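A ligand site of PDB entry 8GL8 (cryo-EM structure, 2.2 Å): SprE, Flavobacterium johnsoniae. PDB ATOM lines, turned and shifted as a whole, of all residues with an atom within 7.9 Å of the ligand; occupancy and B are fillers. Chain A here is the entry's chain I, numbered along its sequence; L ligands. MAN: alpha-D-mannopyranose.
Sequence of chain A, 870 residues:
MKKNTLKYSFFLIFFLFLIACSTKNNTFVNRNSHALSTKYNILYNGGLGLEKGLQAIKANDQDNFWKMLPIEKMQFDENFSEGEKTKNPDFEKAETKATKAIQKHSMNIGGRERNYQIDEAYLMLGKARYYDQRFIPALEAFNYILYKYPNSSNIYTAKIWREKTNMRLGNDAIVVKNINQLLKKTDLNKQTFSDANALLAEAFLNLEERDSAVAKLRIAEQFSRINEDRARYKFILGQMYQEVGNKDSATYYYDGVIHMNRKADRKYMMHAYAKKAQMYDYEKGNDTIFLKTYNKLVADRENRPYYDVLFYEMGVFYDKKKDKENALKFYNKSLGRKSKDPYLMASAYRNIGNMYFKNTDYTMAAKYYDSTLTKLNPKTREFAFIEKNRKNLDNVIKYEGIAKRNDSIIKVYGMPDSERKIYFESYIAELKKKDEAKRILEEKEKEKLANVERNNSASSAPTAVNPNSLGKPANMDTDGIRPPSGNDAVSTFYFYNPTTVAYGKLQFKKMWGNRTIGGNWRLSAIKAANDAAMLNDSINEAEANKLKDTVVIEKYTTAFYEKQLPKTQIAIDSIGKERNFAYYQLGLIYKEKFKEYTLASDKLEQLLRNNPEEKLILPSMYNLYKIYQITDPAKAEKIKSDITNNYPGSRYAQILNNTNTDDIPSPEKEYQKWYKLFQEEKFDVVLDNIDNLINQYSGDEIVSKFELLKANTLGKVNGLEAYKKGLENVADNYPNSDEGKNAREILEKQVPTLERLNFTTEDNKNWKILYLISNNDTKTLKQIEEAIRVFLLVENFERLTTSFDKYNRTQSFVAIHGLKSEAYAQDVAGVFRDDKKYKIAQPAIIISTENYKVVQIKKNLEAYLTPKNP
Hydrophobic or aromatic side chains that line the ligand: Ile 575.
Of the 14 residues printed, 4 come within 4 Å of the ligand.
Along chain A the residues within 4 Å of the ligand span positions 571 to 578.
An oxygen (O2) of the ligand lies within hydrogen-bond range of the backbone carbonyl oxygen of Ala 571, at 3.0 Å.
The side-chain carboxylate (OE2) of Glu 578 sits at hydrogen-bond distance from an oxygen (O4) of the ligand, at 3.4 Å.
O5 of the ligand sits at hydrogen-bond distance from OG of Ser 574, 2.7 Å away.
N of Ile 575 sits close to O2 of the ligand, 3.4 Å away.
ND2 of Asn 406 is in hydrogen-bond range of OE1 of Glu 578 (2.8 Å).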
ATOM      1  N   ILE A 402      16.905  10.832 -22.201  1.00  0.00           N
ATOM      2  CA  ILE A 402      18.067  10.806 -23.091  1.00  0.00           C
ATOM      3  C   ILE A 402      19.310  10.383 -22.316  1.00  0.00           C
ATOM      4  O   ILE A 402      20.061   9.506 -22.741  1.00  0.00           O
ATOM      5  CB  ILE A 402      18.250  12.185 -23.759  1.00  0.00           C
ATOM      6  CG1 ILE A 402      17.299  12.333 -24.940  1.00  0.00           C
ATOM      7  CG2 ILE A 402      19.690  12.367 -24.206  1.00  0.00           C
ATOM      8  CD1 ILE A 402      17.231  13.737 -25.484  1.00  0.00           C
ATOM      9  N   ARG A 405      19.104   6.596 -21.232  1.00  0.00           N
ATOM     10  CA  ARG A 405      19.321   5.629 -22.298  1.00  0.00           C
ATOM     11  C   ARG A 405      20.758   5.677 -22.804  1.00  0.00           C
ATOM     12  O   ARG A 405      21.365   4.624 -23.076  1.00  0.00           O
ATOM     13  CB  ARG A 405      18.317   5.853 -23.432  1.00  0.00           C
ATOM     14  CG  ARG A 405      18.656   6.959 -24.417  1.00  0.00           C
ATOM     15  CD  ARG A 405      17.489   7.234 -25.347  1.00  0.00           C
ATOM     16  NE  ARG A 405      17.160   6.083 -26.180  1.00  0.00           N
ATOM     17  CZ  ARG A 405      17.874   5.684 -27.221  1.00  0.00           C
ATOM     18  NH1 ARG A 405      18.950   6.337 -27.616  1.00  0.00           N
ATOM     19  NH2 ARG A 405      17.490   4.606 -27.907  1.00  0.00           N
ATOM     20  N   ASN A 406      21.350   6.871 -22.898  1.00  0.00           N
ATOM     21  CA  ASN A 406      22.737   6.960 -23.342  1.00  0.00           C
ATOM     22  C   ASN A 406      23.686   6.392 -22.297  1.00  0.00           C
ATOM     23  O   ASN A 406      24.692   5.763 -22.647  1.00  0.00           O
ATOM     24  CB  ASN A 406      23.086   8.404 -23.677  1.00  0.00           C
ATOM     25  CG  ASN A 406      22.451   8.864 -24.973  1.00  0.00           C
ATOM     26  OD1 ASN A 406      22.915   8.518 -26.062  1.00  0.00           O
ATOM     27  ND2 ASN A 406      21.389   9.641 -24.862  1.00  0.00           N
ATOM     28  N   ILE A 409      23.543   2.692 -22.706  1.00  0.00           N
ATOM     29  CA  ILE A 409      24.323   2.301 -23.871  1.00  0.00           C
ATOM     30  C   ILE A 409      25.813   2.317 -23.548  1.00  0.00           C
ATOM     31  O   ILE A 409      26.548   1.390 -23.912  1.00  0.00           O
ATOM     32  CB  ILE A 409      23.997   3.207 -25.071  1.00  0.00           C
ATOM     33  CG1 ILE A 409      22.557   2.984 -25.535  1.00  0.00           C
ATOM     34  CG2 ILE A 409      24.972   2.969 -26.215  1.00  0.00           C
ATOM     35  CD1 ILE A 409      22.268   3.550 -26.915  1.00  0.00           C
ATOM     36  N   PRO A 566      26.084   0.305 -31.470  1.00  0.00           N
ATOM     37  CA  PRO A 566      26.752   1.006 -32.577  1.00  0.00           C
ATOM     38  C   PRO A 566      28.186   0.509 -32.752  1.00  0.00           C
ATOM     39  O   PRO A 566      29.058   0.828 -31.939  1.00  0.00           O
ATOM     40  CB  PRO A 566      26.708   2.474 -32.156  1.00  0.00           C
ATOM     41  CG  PRO A 566      25.807   2.547 -30.959  1.00  0.00           C
ATOM     42  CD  PRO A 566      25.819   1.192 -30.338  1.00  0.00           C
ATOM     43  N   ILE A 570      32.971   6.789 -33.991  1.00  0.00           N
ATOM     44  CA  ILE A 570      32.348   8.114 -34.047  1.00  0.00           C
ATOM     45  C   ILE A 570      30.934   8.057 -33.486  1.00  0.00           C
ATOM     46  O   ILE A 570      30.445   9.040 -32.907  1.00  0.00           O
ATOM     47  CB  ILE A 570      32.395   8.677 -35.477  1.00  0.00           C
ATOM     48  CG1 ILE A 570      31.228   8.151 -36.323  1.00  0.00           C
ATOM     49  CG2 ILE A 570      33.724   8.331 -36.142  1.00  0.00           C
ATOM     50  CD1 ILE A 570      30.825   9.076 -37.450  1.00  0.00           C
ATOM     51  N   ALA A 571      30.248   6.924 -33.647  1.00  0.00           N
ATOM     52  CA  ALA A 571      28.896   6.785 -33.120  1.00  0.00           C
ATOM     53  C   ALA A 571      28.889   6.827 -31.601  1.00  0.00           C
ATOM     54  O   ALA A 571      28.065   7.518 -30.990  1.00  0.00           O
ATOM     55  CB  ALA A 571      28.261   5.497 -33.631  1.00  0.00           C
ATOM     56  N   ILE A 572      29.808   6.101 -30.967  1.00  0.00           N
ATOM     57  CA  ILE A 572      29.872   6.130 -29.507  1.00  0.00           C
ATOM     58  C   ILE A 572      30.363   7.497 -29.023  1.00  0.00           C
ATOM     59  O   ILE A 572      29.976   7.936 -27.939  1.00  0.00           O
ATOM     60  CB  ILE A 572      30.732   4.984 -28.966  1.00  0.00           C
ATOM     61  CG1 ILE A 572      30.485   4.809 -27.467  1.00  0.00           C
ATOM     62  CG2 ILE A 572      32.211   5.213 -29.234  1.00  0.00           C
ATOM     63  CD1 ILE A 572      30.275   3.375 -27.043  1.00  0.00           C
ATOM     64  N   ASP A 573      31.204   8.170 -29.809  1.00  0.00           N
ATOM     65  CA  ASP A 573      31.602   9.526 -29.448  1.00  0.00           C
ATOM     66  C   ASP A 573      30.392  10.459 -29.452  1.00  0.00           C
ATOM     67  O   ASP A 573      30.227  11.277 -28.537  1.00  0.00           O
ATOM     68  CB  ASP A 573      32.686  10.029 -30.402  1.00  0.00           C
ATOM     69  CG  ASP A 573      34.041   9.419 -30.106  1.00  0.00           C
ATOM     70  OD1 ASP A 573      34.221   8.878 -28.999  1.00  0.00           O
ATOM     71  OD2 ASP A 573      34.923   9.483 -30.991  1.00  0.00           O
ATOM     72  N   SER A 574      29.542  10.342 -30.473  1.00  0.00           N
ATOM     73  CA  SER A 574      28.325  11.147 -30.507  1.00  0.00           C
ATOM     74  C   SER A 574      27.383  10.784 -29.369  1.00  0.00           C
ATOM     75  O   SER A 574      26.725  11.666 -28.800  1.00  0.00           O
ATOM     76  CB  SER A 574      27.619  10.969 -31.852  1.00  0.00           C
ATOM     77  OG  SER A 574      26.222  11.194 -31.716  1.00  0.00           O
ATOM     78  N   ILE A 575      27.295   9.500 -29.009  1.00  0.00           N
ATOM     79  CA  ILE A 575      26.445   9.080 -27.902  1.00  0.00           C
ATOM     80  C   ILE A 575      26.946   9.670 -26.588  1.00  0.00           C
ATOM     81  O   ILE A 575      26.157  10.171 -25.776  1.00  0.00           O
ATOM     82  CB  ILE A 575      26.369   7.544 -27.849  1.00  0.00           C
ATOM     83  CG1 ILE A 575      25.258   7.040 -28.775  1.00  0.00           C
ATOM     84  CG2 ILE A 575      26.123   7.066 -26.426  1.00  0.00           C
ATOM     85  CD1 ILE A 575      25.188   5.534 -28.866  1.00  0.00           C
ATOM     86  N   GLY A 576      28.264   9.629 -26.363  1.00  0.00           N
ATOM     87  CA  GLY A 576      28.807  10.245 -25.169  1.00  0.00           C
ATOM     88  C   GLY A 576      28.613  11.751 -25.143  1.00  0.00           C
ATOM     89  O   GLY A 576      28.352  12.341 -24.095  1.00  0.00           O
ATOM     90  N   LYS A 577      28.734  12.397 -26.314  1.00  0.00           N
ATOM     91  CA  LYS A 577      28.460  13.824 -26.404  1.00  0.00           C
ATOM     92  C   LYS A 577      27.016  14.119 -26.029  1.00  0.00           C
ATOM     93  O   LYS A 577      26.737  15.080 -25.290  1.00  0.00           O
ATOM     94  CB  LYS A 577      28.761  14.326 -27.814  1.00  0.00           C
ATOM     95  CG  LYS A 577      28.501  15.808 -28.015  1.00  0.00           C
ATOM     96  CD  LYS A 577      28.950  16.272 -29.393  1.00  0.00           C
ATOM     97  CE  LYS A 577      30.332  15.746 -29.753  1.00  0.00           C
ATOM     98  NZ  LYS A 577      31.345  16.056 -28.708  1.00  0.00           N
ATOM     99  N   GLU A 578      26.078  13.307 -26.524  1.00  0.00           N
ATOM    100  CA  GLU A 578      24.675  13.491 -26.187  1.00  0.00           C
ATOM    101  C   GLU A 578      24.432  13.287 -24.694  1.00  0.00           C
ATOM    102  O   GLU A 578      23.670  14.031 -24.071  1.00  0.00           O
ATOM    103  CB  GLU A 578      23.804  12.543 -27.000  1.00  0.00           C
ATOM    104  CG  GLU A 578      22.318  12.817 -26.890  1.00  0.00           C
ATOM    105  CD  GLU A 578      21.485  11.896 -27.759  1.00  0.00           C
ATOM    106  OE1 GLU A 578      21.510  10.668 -27.508  1.00  0.00           O
ATOM    107  OE2 GLU A 578      20.810  12.385 -28.687  1.00  0.00           O
HETATM  108  C1  MAN L   1      24.722   9.293 -33.937  1.00  0.00           C
HETATM  109  C2  MAN L   1      24.407   8.397 -32.726  1.00  0.00           C
HETATM  110  C3  MAN L   1      23.036   8.733 -32.162  1.00  0.00           C
HETATM  111  C4  MAN L   1      22.903  10.241 -31.916  1.00  0.00           C
HETATM  112  C5  MAN L   1      23.173  10.983 -33.230  1.00  0.00           C
HETATM  113  C6  MAN L   1      23.106  12.494 -33.086  1.00  0.00           C
HETATM  114  O2  MAN L   1      25.328   8.626 -31.660  1.00  0.00           O
HETATM  115  O3  MAN L   1      22.754   8.010 -30.968  1.00  0.00           O
HETATM  116  O4  MAN L   1      21.601  10.552 -31.460  1.00  0.00           O
HETATM  117  O5  MAN L   1      24.502  10.656 -33.675  1.00  0.00           O
HETATM  118  O6  MAN L   1      23.045  13.060 -34.387  1.00  0.00           O
